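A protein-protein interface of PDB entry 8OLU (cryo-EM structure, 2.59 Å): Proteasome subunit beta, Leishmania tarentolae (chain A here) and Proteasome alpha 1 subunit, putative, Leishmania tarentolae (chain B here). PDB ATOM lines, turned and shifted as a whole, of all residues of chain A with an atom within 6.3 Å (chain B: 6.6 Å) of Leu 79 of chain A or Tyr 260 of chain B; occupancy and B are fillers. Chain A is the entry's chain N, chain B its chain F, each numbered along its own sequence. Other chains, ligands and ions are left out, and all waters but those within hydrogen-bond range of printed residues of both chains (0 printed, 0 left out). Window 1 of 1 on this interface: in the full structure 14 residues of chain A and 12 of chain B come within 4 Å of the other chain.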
ATOM      1  N   HIS A  44      26.392  16.209  -9.438  1.00  0.00           N
ATOM      2  CA  HIS A  44      25.436  16.424  -8.369  1.00  0.00           C
ATOM      3  C   HIS A  44      24.472  15.272  -8.160  1.00  0.00           C
ATOM      4  O   HIS A  44      23.529  15.436  -7.459  1.00  0.00           O
ATOM      5  CB  HIS A  44      24.585  17.625  -8.720  1.00  0.00           C
ATOM      6  CG  HIS A  44      25.362  18.835  -9.129  1.00  0.00           C
ATOM      7  ND1 HIS A  44      26.214  19.527  -8.250  1.00  0.00           N
ATOM      8  CD2 HIS A  44      25.356  19.453 -10.374  1.00  0.00           C
ATOM      9  CE1 HIS A  44      26.746  20.538  -8.941  1.00  0.00           C
ATOM     10  NE2 HIS A  44      26.188  20.544 -10.261  1.00  0.00           N
ATOM     11  N   SER A  45      24.614  14.165  -8.854  1.00  0.00           N
ATOM     12  CA  SER A  45      23.537  13.225  -8.871  1.00  0.00           C
ATOM     13  C   SER A  45      24.104  11.824  -8.781  1.00  0.00           C
ATOM     14  O   SER A  45      25.287  11.630  -8.941  1.00  0.00           O
ATOM     15  CB  SER A  45      22.728  13.449 -10.084  1.00  0.00           C
ATOM     16  OG  SER A  45      23.206  14.597 -10.821  1.00  0.00           O
ATOM     17  N   VAL A  63      23.422   8.382 -20.168  1.00  0.00           N
ATOM     18  CA  VAL A  63      23.138   9.601 -19.448  1.00  0.00           C
ATOM     19  C   VAL A  63      24.410  10.278 -19.029  1.00  0.00           C
ATOM     20  O   VAL A  63      24.426  11.459 -19.067  1.00  0.00           O
ATOM     21  CB  VAL A  63      22.280   9.317 -18.209  1.00  0.00           C
ATOM     22  CG1 VAL A  63      22.160  10.515 -17.258  1.00  0.00           C
ATOM     23  CG2 VAL A  63      20.892   8.803 -18.569  1.00  0.00           C
ATOM     24  N   ASN A  66      25.837  12.031 -22.097  1.00  0.00           N
ATOM     25  CA  ASN A  66      25.046  13.176 -22.425  1.00  0.00           C
ATOM     26  C   ASN A  66      25.392  14.323 -21.507  1.00  0.00           C
ATOM     27  O   ASN A  66      25.619  15.420 -21.934  1.00  0.00           O
ATOM     28  CB  ASN A  66      23.597  12.774 -22.326  1.00  0.00           C
ATOM     29  CG  ASN A  66      22.662  13.877 -22.729  1.00  0.00           C
ATOM     30  OD1 ASN A  66      21.966  14.438 -21.893  1.00  0.00           O
ATOM     31  ND2 ASN A  66      22.711  14.230 -23.993  1.00  0.00           N
ATOM     32  N   ILE A  67      25.519  14.064 -20.241  1.00  0.00           N
ATOM     33  CA  ILE A  67      25.842  15.122 -19.317  1.00  0.00           C
ATOM     34  C   ILE A  67      27.200  15.726 -19.602  1.00  0.00           C
ATOM     35  O   ILE A  67      27.384  16.920 -19.486  1.00  0.00           O
ATOM     36  CB  ILE A  67      25.830  14.588 -17.884  1.00  0.00           C
ATOM     37  CG1 ILE A  67      24.441  14.164 -17.487  1.00  0.00           C
ATOM     38  CG2 ILE A  67      26.336  15.589 -16.871  1.00  0.00           C
ATOM     39  CD1 ILE A  67      24.452  13.483 -16.135  1.00  0.00           C
ATOM     40  N   GLN A  70      27.391  17.579 -23.079  1.00  0.00           N
ATOM     41  CA  GLN A  70      26.659  18.824 -23.130  1.00  0.00           C
ATOM     42  C   GLN A  70      27.565  19.885 -22.544  1.00  0.00           C
ATOM     43  O   GLN A  70      27.623  20.966 -23.053  1.00  0.00           O
ATOM     44  CB  GLN A  70      25.324  18.680 -22.401  1.00  0.00           C
ATOM     45  CG  GLN A  70      24.251  19.625 -22.901  1.00  0.00           C
ATOM     46  CD  GLN A  70      23.673  20.576 -21.863  1.00  0.00           C
ATOM     47  OE1 GLN A  70      24.204  20.732 -20.752  1.00  0.00           O
ATOM     48  NE2 GLN A  70      22.589  21.254 -22.247  1.00  0.00           N
ATOM     49  N   LYS A  71      28.349  19.548 -21.555  1.00  0.00           N
ATOM     50  CA  LYS A  71      29.046  20.521 -20.761  1.00  0.00           C
ATOM     51  C   LYS A  71      30.429  20.843 -21.312  1.00  0.00           C
ATOM     52  O   LYS A  71      30.997  21.901 -21.047  1.00  0.00           O
ATOM     53  CB  LYS A  71      29.251  19.818 -19.434  1.00  0.00           C
ATOM     54  CG  LYS A  71      29.952  20.591 -18.345  1.00  0.00           C
ATOM     55  CD  LYS A  71      30.389  19.714 -17.172  1.00  0.00           C
ATOM     56  CE  LYS A  71      30.705  20.650 -16.013  1.00  0.00           C
ATOM     57  NZ  LYS A  71      31.970  20.320 -15.316  1.00  0.00           N
ATOM     58  N   ASP A  77      26.306  25.500 -18.143  1.00  0.00           N
ATOM     59  CA  ASP A  77      26.303  24.926 -16.805  1.00  0.00           C
ATOM     60  C   ASP A  77      25.868  23.478 -16.936  1.00  0.00           C
ATOM     61  O   ASP A  77      24.941  23.182 -17.669  1.00  0.00           O
ATOM     62  CB  ASP A  77      25.350  25.667 -15.858  1.00  0.00           C
ATOM     63  CG  ASP A  77      25.769  27.097 -15.512  1.00  0.00           C
ATOM     64  OD1 ASP A  77      25.508  27.535 -14.368  1.00  0.00           O
ATOM     65  OD2 ASP A  77      26.377  27.769 -16.380  1.00  0.00           O
ATOM     66  N   GLU A  78      26.543  22.599 -16.225  1.00  0.00           N
ATOM     67  CA  GLU A  78      26.072  21.240 -16.077  1.00  0.00           C
ATOM     68  C   GLU A  78      24.562  21.177 -15.824  1.00  0.00           C
ATOM     69  O   GLU A  78      23.961  22.043 -15.220  1.00  0.00           O
ATOM     70  CB  GLU A  78      26.779  20.617 -14.882  1.00  0.00           C
ATOM     71  CG  GLU A  78      26.787  19.110 -14.916  1.00  0.00           C
ATOM     72  CD  GLU A  78      27.625  18.420 -13.851  1.00  0.00           C
ATOM     73  OE1 GLU A  78      28.829  18.803 -13.655  1.00  0.00           O
ATOM     74  OE2 GLU A  78      27.089  17.466 -13.250  1.00  0.00           O
ATOM     75  N   LEU A  79      23.983  20.108 -16.294  1.00  0.00           N
ATOM     76  CA  LEU A  79      22.590  19.880 -16.149  1.00  0.00           C
ATOM     77  C   LEU A  79      22.281  19.713 -14.688  1.00  0.00           C
ATOM     78  O   LEU A  79      23.001  19.036 -13.951  1.00  0.00           O
ATOM     79  CB  LEU A  79      22.262  18.547 -16.801  1.00  0.00           C
ATOM     80  CG  LEU A  79      22.218  18.552 -18.321  1.00  0.00           C
ATOM     81  CD1 LEU A  79      22.135  17.131 -18.823  1.00  0.00           C
ATOM     82  CD2 LEU A  79      21.050  19.387 -18.855  1.00  0.00           C
ATOM     83  N   SER A  80      21.124  20.229 -14.297  1.00  0.00           N
ATOM     84  CA  SER A  80      20.715  20.023 -12.943  1.00  0.00           C
ATOM     85  C   SER A  80      20.278  18.573 -12.765  1.00  0.00           C
ATOM     86  O   SER A  80      20.128  17.778 -13.690  1.00  0.00           O
ATOM     87  CB  SER A  80      19.615  20.947 -12.616  1.00  0.00           C
ATOM     88  OG  SER A  80      18.378  20.432 -13.104  1.00  0.00           O
ATOM     89  N   PRO A  81      20.053  18.173 -11.520  1.00  0.00           N
ATOM     90  CA  PRO A  81      19.473  16.872 -11.256  1.00  0.00           C
ATOM     91  C   PRO A  81      18.108  16.652 -11.848  1.00  0.00           C
ATOM     92  O   PRO A  81      17.860  15.603 -12.358  1.00  0.00           O
ATOM     93  CB  PRO A  81      19.372  16.884  -9.739  1.00  0.00           C
ATOM     94  CG  PRO A  81      20.571  17.655  -9.366  1.00  0.00           C
ATOM     95  CD  PRO A  81      20.555  18.837 -10.314  1.00  0.00           C
ATOM     96  N   SER A  82      17.212  17.602 -11.716  1.00  0.00           N
ATOM     97  CA  SER A  82      15.932  17.399 -12.348  1.00  0.00           C
ATOM     98  C   SER A  82      16.116  17.252 -13.850  1.00  0.00           C
ATOM     99  O   SER A  82      15.502  16.391 -14.450  1.00  0.00           O
ATOM    100  CB  SER A  82      14.956  18.454 -12.003  1.00  0.00           C
ATOM    101  OG  SER A  82      15.617  19.699 -12.009  1.00  0.00           O
ATOM    102  N   GLU A  83      16.982  18.028 -14.456  1.00  0.00           N
ATOM    103  CA  GLU A  83      17.173  17.908 -15.884  1.00  0.00           C
ATOM    104  C   GLU A  83      17.719  16.545 -16.267  1.00  0.00           C
ATOM    105  O   GLU A  83      17.364  15.997 -17.276  1.00  0.00           O
ATOM    106  CB  GLU A  83      18.090  19.039 -16.359  1.00  0.00           C
ATOM    107  CG  GLU A  83      17.481  20.449 -16.378  1.00  0.00           C
ATOM    108  CD  GLU A  83      18.391  21.660 -16.026  1.00  0.00           C
ATOM    109  OE1 GLU A  83      19.641  21.720 -16.507  1.00  0.00           O
ATOM    110  OE2 GLU A  83      17.868  22.629 -15.249  1.00  0.00           O
ATOM    111  N   VAL A  84      18.607  15.985 -15.476  1.00  0.00           N
ATOM    112  CA  VAL A  84      19.181  14.690 -15.785  1.00  0.00           C
ATOM    113  C   VAL A  84      18.160  13.616 -15.606  1.00  0.00           C
ATOM    114  O   VAL A  84      18.051  12.664 -16.352  1.00  0.00           O
ATOM    115  CB  VAL A  84      20.298  14.401 -14.816  1.00  0.00           C
ATOM    116  CG1 VAL A  84      20.806  13.034 -15.003  1.00  0.00           C
ATOM    117  CG2 VAL A  84      21.485  15.315 -15.003  1.00  0.00           C
ATOM    118  N   TYR A  87      15.864  13.715 -18.454  1.00  0.00           N
ATOM    119  CA  TYR A  87      16.438  13.029 -19.574  1.00  0.00           C
ATOM    120  C   TYR A  87      16.375  11.516 -19.481  1.00  0.00           C
ATOM    121  O   TYR A  87      16.196  10.810 -20.446  1.00  0.00           O
ATOM    122  CB  TYR A  87      17.897  13.408 -19.658  1.00  0.00           C
ATOM    123  CG  TYR A  87      18.632  12.678 -20.749  1.00  0.00           C
ATOM    124  CD1 TYR A  87      18.458  13.032 -22.055  1.00  0.00           C
ATOM    125  CD2 TYR A  87      19.412  11.566 -20.491  1.00  0.00           C
ATOM    126  CE1 TYR A  87      19.112  12.386 -23.079  1.00  0.00           C
ATOM    127  CE2 TYR A  87      20.049  10.872 -21.515  1.00  0.00           C
ATOM    128  CZ  TYR A  87      19.945  11.330 -22.811  1.00  0.00           C
ATOM    129  OH  TYR A  87      20.564  10.698 -23.838  1.00  0.00           O
ATOM    130  N   ARG A 112      21.665  20.326  -5.868  1.00  0.00           N
ATOM    131  CA  ARG A 112      22.366  21.469  -6.395  1.00  0.00           C
ATOM    132  C   ARG A 112      21.878  22.762  -5.761  1.00  0.00           C
ATOM    133  O   ARG A 112      20.692  23.080  -5.856  1.00  0.00           O
ATOM    134  CB  ARG A 112      22.184  21.585  -7.901  1.00  0.00           C
ATOM    135  CG  ARG A 112      23.341  22.388  -8.437  1.00  0.00           C
ATOM    136  CD  ARG A 112      23.381  22.463  -9.913  1.00  0.00           C
ATOM    137  NE  ARG A 112      22.072  22.880 -10.355  1.00  0.00           N
ATOM    138  CZ  ARG A 112      21.846  23.245 -11.604  1.00  0.00           C
ATOM    139  NH1 ARG A 112      22.787  22.992 -12.524  1.00  0.00           N
ATOM    140  NH2 ARG A 112      20.710  23.886 -11.862  1.00  0.00           N
ATOM    141  N   THR B 255      11.779  24.227 -32.981  1.00  0.00           N
ATOM    142  CA  THR B 255      11.696  22.807 -32.850  1.00  0.00           C
ATOM    143  C   THR B 255      12.818  22.267 -31.979  1.00  0.00           C
ATOM    144  O   THR B 255      12.572  21.372 -31.182  1.00  0.00           O
ATOM    145  CB  THR B 255      11.835  22.161 -34.216  1.00  0.00           C
ATOM    146  OG1 THR B 255      10.795  22.687 -35.030  1.00  0.00           O
ATOM    147  CG2 THR B 255      11.733  20.666 -34.111  1.00  0.00           C
ATOM    148  N   GLU B 256      14.034  22.791 -32.135  1.00  0.00           N
ATOM    149  CA  GLU B 256      15.116  22.308 -31.321  1.00  0.00           C
ATOM    150  C   GLU B 256      14.918  22.681 -29.862  1.00  0.00           C
ATOM    151  O   GLU B 256      15.130  21.837 -28.975  1.00  0.00           O
ATOM    152  CB  GLU B 256      16.459  22.773 -31.818  1.00  0.00           C
ATOM    153  CG  GLU B 256      16.949  22.016 -33.066  1.00  0.00           C
ATOM    154  CD  GLU B 256      16.775  20.498 -33.200  1.00  0.00           C
ATOM    155  OE1 GLU B 256      17.171  19.715 -32.240  1.00  0.00           O
ATOM    156  OE2 GLU B 256      16.236  20.067 -34.305  1.00  0.00           O
ATOM    157  N   CYS B 257      14.410  23.868 -29.610  1.00  0.00           N
ATOM    158  CA  CYS B 257      14.047  24.214 -28.274  1.00  0.00           C
ATOM    159  C   CYS B 257      12.919  23.404 -27.703  1.00  0.00           C
ATOM    160  O   CYS B 257      12.852  23.236 -26.507  1.00  0.00           O
ATOM    161  CB  CYS B 257      13.609  25.643 -28.161  1.00  0.00           C
ATOM    162  SG  CYS B 257      15.066  26.700 -28.291  1.00  0.00           S
ATOM    163  N   MET B 258      11.960  22.976 -28.462  1.00  0.00           N
ATOM    164  CA  MET B 258      10.967  22.133 -27.838  1.00  0.00           C
ATOM    165  C   MET B 258      11.573  20.761 -27.589  1.00  0.00           C
ATOM    166  O   MET B 258      11.247  20.194 -26.581  1.00  0.00           O
ATOM    167  CB  MET B 258       9.755  21.966 -28.745  1.00  0.00           C
ATOM    168  CG  MET B 258       8.940  23.231 -28.910  1.00  0.00           C
ATOM    169  SD  MET B 258       7.579  22.876 -30.018  1.00  0.00           S
ATOM    170  CE  MET B 258       7.197  24.458 -30.774  1.00  0.00           C
ATOM    171  N   ASN B 259      12.390  20.211 -28.496  1.00  0.00           N
ATOM    172  CA  ASN B 259      12.944  18.924 -28.204  1.00  0.00           C
ATOM    173  C   ASN B 259      13.736  19.025 -26.912  1.00  0.00           C
ATOM    174  O   ASN B 259      13.591  18.205 -25.994  1.00  0.00           O
ATOM    175  CB  ASN B 259      13.849  18.321 -29.262  1.00  0.00           C
ATOM    176  CG  ASN B 259      13.200  18.270 -30.643  1.00  0.00           C
ATOM    177  OD1 ASN B 259      11.962  18.255 -30.779  1.00  0.00           O
ATOM    178  ND2 ASN B 259      14.042  18.276 -31.687  1.00  0.00           N
ATOM    179  N   TYR B 260      14.521  20.094 -26.799  1.00  0.00           N
ATOM    180  CA  TYR B 260      15.355  20.173 -25.636  1.00  0.00           C
ATOM    181  C   TYR B 260      14.493  20.296 -24.421  1.00  0.00           C
ATOM    182  O   TYR B 260      14.783  19.723 -23.425  1.00  0.00           O
ATOM    183  CB  TYR B 260      16.233  21.392 -25.680  1.00  0.00           C
ATOM    184  CG  TYR B 260      17.221  21.461 -24.582  1.00  0.00           C
ATOM    185  CD1 TYR B 260      18.516  21.042 -24.741  1.00  0.00           C
ATOM    186  CD2 TYR B 260      16.844  21.960 -23.369  1.00  0.00           C
ATOM    187  CE1 TYR B 260      19.430  21.110 -23.691  1.00  0.00           C
ATOM    188  CE2 TYR B 260      17.759  22.091 -22.332  1.00  0.00           C
ATOM    189  CZ  TYR B 260      19.068  21.672 -22.483  1.00  0.00           C
ATOM    190  OH  TYR B 260      19.866  21.801 -21.393  1.00  0.00           O
ATOM    191  N   ARG B 261      13.444  21.058 -24.467  1.00  0.00           N
ATOM    192  CA  ARG B 261      12.691  21.242 -23.252  1.00  0.00           C
ATOM    193  C   ARG B 261      11.909  20.018 -22.926  1.00  0.00           C
ATOM    194  O   ARG B 261      11.719  19.742 -21.794  1.00  0.00           O
ATOM    195  CB  ARG B 261      11.711  22.352 -23.485  1.00  0.00           C
ATOM    196  CG  ARG B 261      10.871  22.645 -22.281  1.00  0.00           C
ATOM    197  CD  ARG B 261      10.188  23.973 -22.487  1.00  0.00           C
ATOM    198  NE  ARG B 261      11.212  24.973 -22.429  1.00  0.00           N
ATOM    199  CZ  ARG B 261      11.396  25.693 -21.343  1.00  0.00           C
ATOM    200  NH1 ARG B 261      11.033  25.235 -20.144  1.00  0.00           N
ATOM    201  NH2 ARG B 261      11.999  26.864 -21.481  1.00  0.00           N
ATOM    202  N   TYR B 262      11.467  19.295 -23.929  1.00  0.00           N
ATOM    203  CA  TYR B 262      10.890  17.991 -23.712  1.00  0.00           C
ATOM    204  C   TYR B 262      11.859  17.083 -22.986  1.00  0.00           C
ATOM    205  O   TYR B 262      11.454  16.357 -22.111  1.00  0.00           O
ATOM    206  CB  TYR B 262      10.589  17.313 -25.038  1.00  0.00           C
ATOM    207  CG  TYR B 262      10.119  15.906 -24.961  1.00  0.00           C
ATOM    208  CD1 TYR B 262       8.880  15.609 -24.443  1.00  0.00           C
ATOM    209  CD2 TYR B 262      10.919  14.864 -25.386  1.00  0.00           C
ATOM    210  CE1 TYR B 262       8.471  14.272 -24.323  1.00  0.00           C
ATOM    211  CE2 TYR B 262      10.535  13.525 -25.289  1.00  0.00           C
ATOM    212  CZ  TYR B 262       9.289  13.236 -24.781  1.00  0.00           C
ATOM    213  OH  TYR B 262       8.845  11.985 -24.712  1.00  0.00           O
ATOM    214  N   MET B 263      13.105  17.032 -23.411  1.00  0.00           N
ATOM    215  CA  MET B 263      14.005  16.070 -22.839  1.00  0.00           C
ATOM    216  C   MET B 263      14.412  16.509 -21.465  1.00  0.00           C
ATOM    217  O   MET B 263      14.331  15.721 -20.559  1.00  0.00           O
ATOM    218  CB  MET B 263      15.258  15.911 -23.680  1.00  0.00           C
ATOM    219  CG  MET B 263      14.955  15.183 -24.966  1.00  0.00           C
ATOM    220  SD  MET B 263      14.390  13.466 -24.756  1.00  0.00           S
ATOM    221  CE  MET B 263      15.900  12.966 -23.946  1.00  0.00           C
ATOM    222  N   TYR B 264      14.835  17.724 -21.290  1.00  0.00           N
ATOM    223  CA  TYR B 264      15.432  18.058 -20.031  1.00  0.00           C
ATOM    224  C   TYR B 264      14.524  18.871 -19.149  1.00  0.00           C
ATOM    225  O   TYR B 264      14.948  19.352 -18.111  1.00  0.00           O
ATOM    226  CB  TYR B 264      16.690  18.885 -20.253  1.00  0.00           C
ATOM    227  CG  TYR B 264      17.679  18.143 -21.095  1.00  0.00           C
ATOM    228  CD1 TYR B 264      18.496  17.168 -20.577  1.00  0.00           C
ATOM    229  CD2 TYR B 264      17.708  18.347 -22.443  1.00  0.00           C
ATOM    230  CE1 TYR B 264      19.377  16.464 -21.367  1.00  0.00           C
ATOM    231  CE2 TYR B 264      18.566  17.662 -23.266  1.00  0.00           C
ATOM    232  CZ  TYR B 264      19.416  16.710 -22.719  1.00  0.00           C
ATOM    233  OH  TYR B 264      20.216  16.043 -23.608  1.00  0.00           O
ATOM    234  N   SER B 265      13.309  19.103 -19.572  1.00  0.00           N
ATOM    235  CA  SER B 265      12.371  19.891 -18.787  1.00  0.00           C
ATOM    236  C   SER B 265      12.946  21.204 -18.365  1.00  0.00           C
ATOM    237  O   SER B 265      12.528  21.687 -17.366  1.00  0.00           O
ATOM    238  CB  SER B 265      11.891  19.163 -17.553  1.00  0.00           C
ATOM    239  OG  SER B 265      11.165  17.958 -17.899  1.00  0.00           O
ATOM    240  N   ASN B 266      13.834  21.794 -19.128  1.00  0.00           N
ATOM    241  CA  ASN B 266      14.273  23.148 -18.871  1.00  0.00           C
ATOM    242  C   ASN B 266      14.599  23.771 -20.218  1.00  0.00           C
ATOM    243  O   ASN B 266      14.477  23.130 -21.214  1.00  0.00           O
ATOM    244  CB  ASN B 266      15.472  23.144 -17.959  1.00  0.00           C
ATOM    245  CG  ASN B 266      15.885  24.513 -17.475  1.00  0.00           C
ATOM    246  OD1 ASN B 266      15.114  25.470 -17.476  1.00  0.00           O
ATOM    247  ND2 ASN B 266      17.138  24.633 -17.089  1.00  0.00           N
ATOM    248  N   GLY B 267      14.811  25.072 -20.284  1.00  0.00           N
ATOM    249  CA  GLY B 267      15.078  25.712 -21.550  1.00  0.00           C
ATOM    250  C   GLY B 267      16.438  25.329 -22.121  1.00  0.00           C
ATOM    251  O   GLY B 267      17.369  25.145 -21.386  1.00  0.00           O
ATOM    252  N   MET B 268      16.586  25.287 -23.440  1.00  0.00           N
ATOM    253  CA  MET B 268      17.896  25.071 -24.035  1.00  0.00           C
ATOM    254  C   MET B 268      18.742  26.289 -23.772  1.00  0.00           C
ATOM    255  O   MET B 268      18.259  27.388 -23.945  1.00  0.00           O
ATOM    256  CB  MET B 268      17.883  24.890 -25.547  1.00  0.00           C
ATOM    257  CG  MET B 268      19.279  24.731 -26.070  1.00  0.00           C
ATOM    258  SD  MET B 268      19.394  24.494 -27.833  1.00  0.00           S
ATOM    259  CE  MET B 268      18.383  23.054 -28.122  1.00  0.00           C
ATOM    260  N   PRO B 269      19.926  26.083 -23.187  1.00  0.00           N
ATOM    261  CA  PRO B 269      20.840  27.136 -22.848  1.00  0.00           C
ATOM    262  C   PRO B 269      21.301  27.856 -24.082  1.00  0.00           C
ATOM    263  O   PRO B 269      21.599  27.206 -25.049  1.00  0.00           O
ATOM    264  CB  PRO B 269      22.100  26.446 -22.310  1.00  0.00           C
ATOM    265  CG  PRO B 269      21.655  25.097 -21.920  1.00  0.00           C
ATOM    266  CD  PRO B 269      20.418  24.792 -22.723  1.00  0.00           C
ATOM    267  N   GLN B 272      24.503  26.818 -26.138  1.00  0.00           N
ATOM    268  CA  GLN B 272      24.217  25.660 -26.944  1.00  0.00           C
ATOM    269  C   GLN B 272      23.284  26.001 -28.099  1.00  0.00           C
ATOM    270  O   GLN B 272      23.314  25.367 -29.140  1.00  0.00           O
ATOM    271  CB  GLN B 272      23.582  24.581 -26.054  1.00  0.00           C
ATOM    272  CG  GLN B 272      23.169  23.283 -26.739  1.00  0.00           C
ATOM    273  CD  GLN B 272      22.762  22.249 -25.731  1.00  0.00           C
ATOM    274  OE1 GLN B 272      22.975  22.431 -24.533  1.00  0.00           O
ATOM    275  NE2 GLN B 272      22.196  21.141 -26.185  1.00  0.00           N
ATOM    276  N   MET B 276      24.253  25.583 -32.220  1.00  0.00           N
ATOM    277  CA  MET B 276      23.366  24.935 -33.146  1.00  0.00           C
ATOM    278  C   MET B 276      23.013  25.782 -34.351  1.00  0.00           C
ATOM    279  O   MET B 276      22.919  25.288 -35.454  1.00  0.00           O
ATOM    280  CB  MET B 276      22.049  24.740 -32.438  1.00  0.00           C
ATOM    281  CG  MET B 276      21.813  23.381 -32.019  1.00  0.00           C
ATOM    282  SD  MET B 276      20.018  23.405 -31.772  1.00  0.00           S
ATOM    283  CE  MET B 276      20.016  21.868 -30.825  1.00  0.00           C
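The side-chain amide nitrogen of Gln 70 of chain A sits at hydrogen-bond distance from the side-chain hydroxyl of Tyr 260 of chain B (2.9 Å).
The side-chain amide nitrogen (ND2) of Asn 266 of chain B lies within hydrogen-bond range of the side-chain carboxylate (OE2) of Glu 83 of chain A (2.8 Å).
The side-chain amide oxygen of Asn 66 of chain A lies within hydrogen-bond range of the side-chain hydroxyl of Tyr 264 of chain B (2.9 Å).
The side-chain amide oxygen (OE1) of Gln 272 of chain B is in hydrogen-bond range of the side-chain amide nitrogen (NE2) of Gln 70 of chain A, at 2.6 Å.
The backbone carbonyl oxygen of Met 263 of chain B is in hydrogen-bond range of the backbone NH of Tyr 87 of chain A.
The backbone NH of Ser 80 of chain A lies within hydrogen-bond range of the side-chain carboxylate of Glu 83 of chain A (3.1 Å).
Among the printed residues, merely in contact across the chains: Glu 83 of chain A with Tyr 264 of chain B, Tyr 87 of chain A with Tyr 264 of chain B, Leu 79 of chain A with Tyr 260 of chain B, Leu 79 of chain A with Tyr 264 of chain B and Gln 70 of chain A with Pro 269 of chain B.
Of the printed residues of chain B, Gln 70 of chain A touches Tyr 260, Pro 269 and Gln 272.
Of chain B, only Tyr 260 and Tyr 264 come within 4 Å of Leu 79 of chain A.
Of the printed residues of chain A, Tyr 260 of chain B touches Gln 70 and Leu 79.
Printed residues of chain A within 4 Å of Pro 269 of chain B: Gln 70 (3.97 Å).
Of the printed residues of chain A, Gln 272 of chain B touches Gln 70 (2.6 Å).
The nearest residue of chain A that does not touch Tyr 260 of chain B is Glu 83 of chain A (4.9 Å).
Of the 17 printed residues of chain B, 6 touch a printed residue of chain A.
Hydrophobic or aromatic side chains of chain A that line the printed part of chain B: Leu 79 and Tyr 87.
Among the printed residues, 10 pairs touch across the chains.
Among the printed residues, no Asp or Glu carboxylate lies within 4 Å of a Lys or Arg side-chain nitrogen of the other chain.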
